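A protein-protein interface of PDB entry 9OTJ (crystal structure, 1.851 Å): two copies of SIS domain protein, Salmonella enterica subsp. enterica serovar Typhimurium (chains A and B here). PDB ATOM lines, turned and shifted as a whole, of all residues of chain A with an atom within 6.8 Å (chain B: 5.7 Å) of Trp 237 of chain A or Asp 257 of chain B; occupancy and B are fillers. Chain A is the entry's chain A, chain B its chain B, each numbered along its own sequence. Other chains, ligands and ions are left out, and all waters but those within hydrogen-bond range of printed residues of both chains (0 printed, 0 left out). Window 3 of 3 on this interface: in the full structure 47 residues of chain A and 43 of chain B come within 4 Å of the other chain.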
ATOM      1  N   LYS A 210      -7.402  14.742  32.397  1.00  0.00           N
ATOM      2  CA  LYS A 210      -6.965  15.954  31.710  1.00  0.00           C
ATOM      3  C   LYS A 210      -8.168  16.815  31.314  1.00  0.00           C
ATOM      4  O   LYS A 210      -8.072  18.048  31.290  1.00  0.00           O
ATOM      5  CB  LYS A 210      -6.116  15.636  30.470  1.00  0.00           C
ATOM      6  N   VAL A 211      -9.275  16.143  30.963  1.00  0.00           N
ATOM      7  CA  VAL A 211     -10.515  16.810  30.601  1.00  0.00           C
ATOM      8  C   VAL A 211     -11.653  16.120  31.351  1.00  0.00           C
ATOM      9  O   VAL A 211     -11.553  14.941  31.704  1.00  0.00           O
ATOM     10  CB  VAL A 211     -10.778  16.868  29.077  1.00  0.00           C
ATOM     11  CG1 VAL A 211      -9.569  17.408  28.310  1.00  0.00           C
ATOM     12  CG2 VAL A 211     -11.224  15.526  28.506  1.00  0.00           C
ATOM     13  N   ILE A 231     -13.270  24.392  35.476  1.00  0.00           N
ATOM     14  CA  ILE A 231     -12.470  23.214  35.190  1.00  0.00           C
ATOM     15  C   ILE A 231     -11.335  23.540  34.205  1.00  0.00           C
ATOM     16  O   ILE A 231     -10.199  23.157  34.458  1.00  0.00           O
ATOM     17  CB  ILE A 231     -13.379  22.080  34.691  1.00  0.00           C
ATOM     18  CG1 ILE A 231     -14.129  21.428  35.868  1.00  0.00           C
ATOM     19  CG2 ILE A 231     -12.591  21.065  33.854  1.00  0.00           C
ATOM     20  CD1 ILE A 231     -15.231  20.470  35.442  1.00  0.00           C
ATOM     21  N   PHE A 232     -11.637  24.198  33.071  1.00  0.00           N
ATOM     22  CA  PHE A 232     -10.648  24.510  32.049  1.00  0.00           C
ATOM     23  C   PHE A 232      -9.546  25.400  32.641  1.00  0.00           C
ATOM     24  O   PHE A 232      -8.374  25.231  32.309  1.00  0.00           O
ATOM     25  CB  PHE A 232     -11.334  25.175  30.842  1.00  0.00           C
ATOM     26  CG  PHE A 232     -10.346  25.820  29.874  1.00  0.00           C
ATOM     27  CD1 PHE A 232      -9.302  25.076  29.323  1.00  0.00           C
ATOM     28  CD2 PHE A 232     -10.405  27.181  29.588  1.00  0.00           C
ATOM     29  CE1 PHE A 232      -8.380  25.665  28.465  1.00  0.00           C
ATOM     30  CE2 PHE A 232      -9.475  27.767  28.734  1.00  0.00           C
ATOM     31  CZ  PHE A 232      -8.466  27.009  28.175  1.00  0.00           C
ATOM     32  N   GLU A 234      -8.569  25.257  35.594  1.00  0.00           N
ATOM     33  CA  GLU A 234      -7.800  24.369  36.460  1.00  0.00           C
ATOM     34  C   GLU A 234      -6.894  23.440  35.637  1.00  0.00           C
ATOM     35  O   GLU A 234      -5.698  23.351  35.918  1.00  0.00           O
ATOM     36  CB  GLU A 234      -8.779  23.585  37.343  1.00  0.00           C
ATOM     37  CG  GLU A 234      -8.110  22.812  38.473  1.00  0.00           C
ATOM     38  CD  GLU A 234      -7.092  23.679  39.195  1.00  0.00           C
ATOM     39  OE1 GLU A 234      -7.464  24.721  39.780  1.00  0.00           O
ATOM     40  OE2 GLU A 234      -5.902  23.319  39.131  1.00  0.00           O
ATOM     41  N   MET A 235      -7.474  22.728  34.651  1.00  0.00           N
ATOM     42  CA  MET A 235      -6.757  21.794  33.782  1.00  0.00           C
ATOM     43  C   MET A 235      -5.762  22.545  32.899  1.00  0.00           C
ATOM     44  O   MET A 235      -4.605  22.158  32.808  1.00  0.00           O
ATOM     45  CB  MET A 235      -7.678  21.048  32.796  1.00  0.00           C
ATOM     46  CG  MET A 235      -8.844  20.311  33.413  1.00  0.00           C
ATOM     47  SD  MET A 235      -8.312  19.262  34.779  1.00  0.00           S
ATOM     48  CE  MET A 235      -9.555  17.970  34.641  1.00  0.00           C
ATOM     49  N   GLN A 236      -6.262  23.583  32.213  1.00  0.00           N
ATOM     50  CA  GLN A 236      -5.533  24.341  31.208  1.00  0.00           C
ATOM     51  C   GLN A 236      -5.037  23.451  30.065  1.00  0.00           C
ATOM     52  O   GLN A 236      -3.927  23.667  29.583  1.00  0.00           O
ATOM     53  CB  GLN A 236      -4.378  25.087  31.868  1.00  0.00           C
ATOM     54  CG  GLN A 236      -4.807  25.903  33.079  1.00  0.00           C
ATOM     55  CD  GLN A 236      -3.866  27.050  33.360  1.00  0.00           C
ATOM     56  OE1 GLN A 236      -3.553  27.857  32.476  1.00  0.00           O
ATOM     57  NE2 GLN A 236      -3.400  27.118  34.598  1.00  0.00           N
ATOM     58  N   TRP A 237      -5.853  22.474  29.623  1.00  0.00           N
ATOM     59  CA  TRP A 237      -5.516  21.663  28.459  1.00  0.00           C
ATOM     60  C   TRP A 237      -6.487  21.980  27.318  1.00  0.00           C
ATOM     61  O   TRP A 237      -6.095  22.693  26.392  1.00  0.00           O
ATOM     62  CB  TRP A 237      -5.463  20.156  28.786  1.00  0.00           C
ATOM     63  CG  TRP A 237      -4.689  19.342  27.772  1.00  0.00           C
ATOM     64  CD1 TRP A 237      -5.170  18.296  27.033  1.00  0.00           C
ATOM     65  CD2 TRP A 237      -3.290  19.480  27.402  1.00  0.00           C
ATOM     66  NE1 TRP A 237      -4.189  17.798  26.214  1.00  0.00           N
ATOM     67  CE2 TRP A 237      -3.023  18.493  26.422  1.00  0.00           C
ATOM     68  CE3 TRP A 237      -2.241  20.331  27.792  1.00  0.00           C
ATOM     69  CZ2 TRP A 237      -1.761  18.338  25.841  1.00  0.00           C
ATOM     70  CZ3 TRP A 237      -0.996  20.171  27.216  1.00  0.00           C
ATOM     71  CH2 TRP A 237      -0.759  19.187  26.256  1.00  0.00           C
ATOM     72  N   ILE A 238      -7.735  21.471  27.407  1.00  0.00           N
ATOM     73  CA  ILE A 238      -8.774  21.663  26.397  1.00  0.00           C
ATOM     74  C   ILE A 238     -10.068  22.090  27.101  1.00  0.00           C
ATOM     75  O   ILE A 238     -10.479  21.446  28.077  1.00  0.00           O
ATOM     76  CB  ILE A 238      -8.990  20.381  25.559  1.00  0.00           C
ATOM     77  CG1 ILE A 238      -7.734  19.981  24.767  1.00  0.00           C
ATOM     78  CG2 ILE A 238     -10.215  20.498  24.642  1.00  0.00           C
ATOM     79  CD1 ILE A 238      -7.723  18.524  24.336  1.00  0.00           C
ATOM     80  N   HIS A 239     -10.706  23.162  26.584  1.00  0.00           N
ATOM     81  CA  HIS A 239     -12.003  23.611  27.077  1.00  0.00           C
ATOM     82  C   HIS A 239     -13.056  22.538  26.770  1.00  0.00           C
ATOM     83  O   HIS A 239     -13.481  22.366  25.621  1.00  0.00           O
ATOM     84  CB  HIS A 239     -12.356  25.039  26.622  1.00  0.00           C
ATOM     85  CG  HIS A 239     -13.674  25.550  27.161  1.00  0.00           C
ATOM     86  ND1 HIS A 239     -14.524  26.374  26.452  1.00  0.00           N
ATOM     87  CD2 HIS A 239     -14.299  25.324  28.337  1.00  0.00           C
ATOM     88  CE1 HIS A 239     -15.610  26.622  27.172  1.00  0.00           C
ATOM     89  NE2 HIS A 239     -15.496  25.992  28.321  1.00  0.00           N
ATOM     90  N   TYR A 339      -0.414  30.081  32.243  1.00  0.00           N
ATOM     91  CA  TYR A 339      -1.515  30.931  31.701  1.00  0.00           C
ATOM     92  C   TYR A 339      -2.444  31.277  32.860  1.00  0.00           C
ATOM     93  O   TYR A 339      -3.006  30.381  33.485  1.00  0.00           O
ATOM     94  CB  TYR A 339      -2.282  30.252  30.557  1.00  0.00           C
ATOM     95  CG  TYR A 339      -1.352  29.584  29.557  1.00  0.00           C
ATOM     96  CD1 TYR A 339      -0.697  30.334  28.584  1.00  0.00           C
ATOM     97  CD2 TYR A 339      -1.073  28.220  29.632  1.00  0.00           C
ATOM     98  CE1 TYR A 339       0.190  29.744  27.698  1.00  0.00           C
ATOM     99  CE2 TYR A 339      -0.186  27.621  28.753  1.00  0.00           C
ATOM    100  CZ  TYR A 339       0.446  28.386  27.782  1.00  0.00           C
ATOM    101  OH  TYR A 339       1.319  27.816  26.902  1.00  0.00           O
ATOM    102  N   TRP A 341      -5.741  33.362  33.302  1.00  0.00           N
ATOM    103  CA  TRP A 341      -6.874  34.057  32.714  1.00  0.00           C
ATOM    104  C   TRP A 341      -7.799  34.547  33.830  1.00  0.00           C
ATOM    105  O   TRP A 341      -8.500  33.744  34.451  1.00  0.00           O
ATOM    106  CB  TRP A 341      -7.634  33.138  31.746  1.00  0.00           C
ATOM    107  CG  TRP A 341      -6.794  32.354  30.766  1.00  0.00           C
ATOM    108  CD1 TRP A 341      -6.189  32.834  29.641  1.00  0.00           C
ATOM    109  CD2 TRP A 341      -6.537  30.927  30.780  1.00  0.00           C
ATOM    110  NE1 TRP A 341      -5.543  31.823  28.974  1.00  0.00           N
ATOM    111  CE2 TRP A 341      -5.744  30.640  29.643  1.00  0.00           C
ATOM    112  CE3 TRP A 341      -6.885  29.872  31.637  1.00  0.00           C
ATOM    113  CZ2 TRP A 341      -5.303  29.347  29.351  1.00  0.00           C
ATOM    114  CZ3 TRP A 341      -6.452  28.595  31.340  1.00  0.00           C
ATOM    115  CH2 TRP A 341      -5.672  28.336  30.211  1.00  0.00           C
ATOM    116  N   TYR B 213     -10.823  23.450  17.353  1.00  0.00           N
ATOM    117  CA  TYR B 213     -11.941  24.272  17.794  1.00  0.00           C
ATOM    118  C   TYR B 213     -12.622  24.939  16.585  1.00  0.00           C
ATOM    119  O   TYR B 213     -12.069  25.019  15.476  1.00  0.00           O
ATOM    120  CB  TYR B 213     -11.523  25.379  18.774  1.00  0.00           C
ATOM    121  CG  TYR B 213     -11.012  25.040  20.174  1.00  0.00           C
ATOM    122  CD1 TYR B 213     -11.832  24.455  21.139  1.00  0.00           C
ATOM    123  CD2 TYR B 213      -9.735  25.435  20.576  1.00  0.00           C
ATOM    124  CE1 TYR B 213     -11.365  24.192  22.422  1.00  0.00           C
ATOM    125  CE2 TYR B 213      -9.258  25.191  21.854  1.00  0.00           C
ATOM    126  CZ  TYR B 213     -10.074  24.568  22.784  1.00  0.00           C
ATOM    127  OH  TYR B 213      -9.585  24.349  24.049  1.00  0.00           O
ATOM    128  N   ILE B 255      -6.221  28.892  24.944  1.00  0.00           N
ATOM    129  CA  ILE B 255      -4.871  29.043  24.437  1.00  0.00           C
ATOM    130  C   ILE B 255      -3.922  28.496  25.494  1.00  0.00           C
ATOM    131  O   ILE B 255      -3.720  29.112  26.540  1.00  0.00           O
ATOM    132  CB  ILE B 255      -4.598  30.509  24.058  1.00  0.00           C
ATOM    133  CG1 ILE B 255      -5.281  30.834  22.711  1.00  0.00           C
ATOM    134  CG2 ILE B 255      -3.094  30.817  24.045  1.00  0.00           C
ATOM    135  CD1 ILE B 255      -5.092  32.264  22.240  1.00  0.00           C
ATOM    136  N   THR B 256      -3.395  27.301  25.203  1.00  0.00           N
ATOM    137  CA  THR B 256      -2.678  26.487  26.171  1.00  0.00           C
ATOM    138  C   THR B 256      -1.595  25.706  25.420  1.00  0.00           C
ATOM    139  O   THR B 256      -1.312  25.999  24.255  1.00  0.00           O
ATOM    140  CB  THR B 256      -3.658  25.573  26.926  1.00  0.00           C
ATOM    141  OG1 THR B 256      -3.927  24.379  26.191  1.00  0.00           O
ATOM    142  CG2 THR B 256      -4.993  26.223  27.270  1.00  0.00           C
ATOM    143  N   ASP B 257      -1.011  24.703  26.086  1.00  0.00           N
ATOM    144  CA  ASP B 257       0.093  23.932  25.528  1.00  0.00           C
ATOM    145  C   ASP B 257      -0.402  22.968  24.453  1.00  0.00           C
ATOM    146  O   ASP B 257       0.369  22.587  23.574  1.00  0.00           O
ATOM    147  CB  ASP B 257       0.839  23.152  26.601  1.00  0.00           C
ATOM    148  CG  ASP B 257       1.811  23.940  27.469  1.00  0.00           C
ATOM    149  OD1 ASP B 257       1.974  25.161  27.233  1.00  0.00           O
ATOM    150  OD2 ASP B 257       2.403  23.316  28.378  1.00  0.00           O
ATOM    151  N   ALA B 258      -1.681  22.576  24.529  1.00  0.00           N
ATOM    152  CA  ALA B 258      -2.245  21.597  23.610  1.00  0.00           C
ATOM    153  C   ALA B 258      -2.102  22.045  22.151  1.00  0.00           C
ATOM    154  O   ALA B 258      -2.084  21.200  21.254  1.00  0.00           O
ATOM    155  CB  ALA B 258      -3.695  21.325  23.971  1.00  0.00           C
ATOM    156  N   ASN B 259      -2.031  23.370  21.920  1.00  0.00           N
ATOM    157  CA  ASN B 259      -1.769  23.958  20.607  1.00  0.00           C
ATOM    158  C   ASN B 259      -2.896  23.643  19.614  1.00  0.00           C
ATOM    159  O   ASN B 259      -2.690  23.704  18.394  1.00  0.00           O
ATOM    160  CB  ASN B 259      -0.377  23.580  20.105  1.00  0.00           C
ATOM    161  CG  ASN B 259       0.618  24.702  20.283  1.00  0.00           C
ATOM    162  OD1 ASN B 259       0.715  25.304  21.364  1.00  0.00           O
ATOM    163  ND2 ASN B 259       1.339  25.011  19.214  1.00  0.00           N
ATOM    164  N   THR B 260      -4.087  23.366  20.170  1.00  0.00           N
ATOM    165  CA  THR B 260      -5.319  23.100  19.440  1.00  0.00           C
ATOM    166  C   THR B 260      -5.468  24.101  18.286  1.00  0.00           C
ATOM    167  O   THR B 260      -5.525  25.302  18.540  1.00  0.00           O
ATOM    168  CB  THR B 260      -6.491  23.226  20.432  1.00  0.00           C
ATOM    169  OG1 THR B 260      -6.088  22.783  21.733  1.00  0.00           O
ATOM    170  CG2 THR B 260      -7.744  22.498  19.964  1.00  0.00           C
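OG1 of Thr 256 of chain B lies close to O of Gln 236 of chain A (3.5 Å). The backbone carbonyl oxygen (O) of Trp 237 of chain A lies within hydrogen-bond range of the side-chain hydroxyl (OG1) of Thr 256 of chain B (2.8 Å). N of His 239 of chain A sits at hydrogen-bond distance from OH of Tyr 213 of chain B (3.0 Å). OD1 of Asp 257 of chain B lies within hydrogen-bond range of OH of Tyr 339 of chain A (2.8 Å).
OE1 of Gln 236 of chain A lies close to O of Tyr 339 of chain A. OG1 of Thr 256 of chain B sits close to N of Ala 258 of chain B, 3.3 Å away.
Among the printed residues, merely in contact across the chains: Phe 232 of chain A with Thr 256 of chain B, Trp 237 of chain A with Asp 257 of chain B, Trp 237 of chain A with Ala 258 of chain B, Ile 238 of chain A with Tyr 213 of chain B, Tyr 339 of chain A with Ile 255 of chain B, Tyr 339 of chain A with Thr 256 of chain B, Trp 341 of chain A with Ile 255 of chain B and Trp 341 of chain A with Thr 256 of chain B.
Of the printed residues of chain B, Gln 236 of chain A touches Thr 256 (3.3 Å). Printed residues of chain B within 4 Å of Tyr 339 of chain A: Ile 255 (3.8 Å), Thr 256 (3.8 Å) and Asp 257 (2.8 Å). Of chain A, only Trp 237 and Tyr 339 come within 4 Å of Asp 257 of chain B. The nearest residue of chain B that does not touch Trp 237 of chain A is Tyr 213 of chain B (4.5 Å). The nearest residue of chain A that does not touch Asp 257 of chain B is Gln 236 of chain A (4.7 Å).
Printed residues of chain B that touch a printed residue of chain A: Tyr 213, Ile 255, Thr 256, Asp 257 and Ala 258. Hydrophobic or aromatic side chains of chain B that line the printed part of chain A: Tyr 213 and Ala 258. Of the 12 printed residues of chain A, 7 touch a printed residue of chain B. Along chain A the printed residues that touch a printed residue of chain B span positions 232 to 341.
No position is printed for both chains. Of the 12 pairs that touch across the chains among the printed residues, none has its exchanged pair printed and touching as well.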
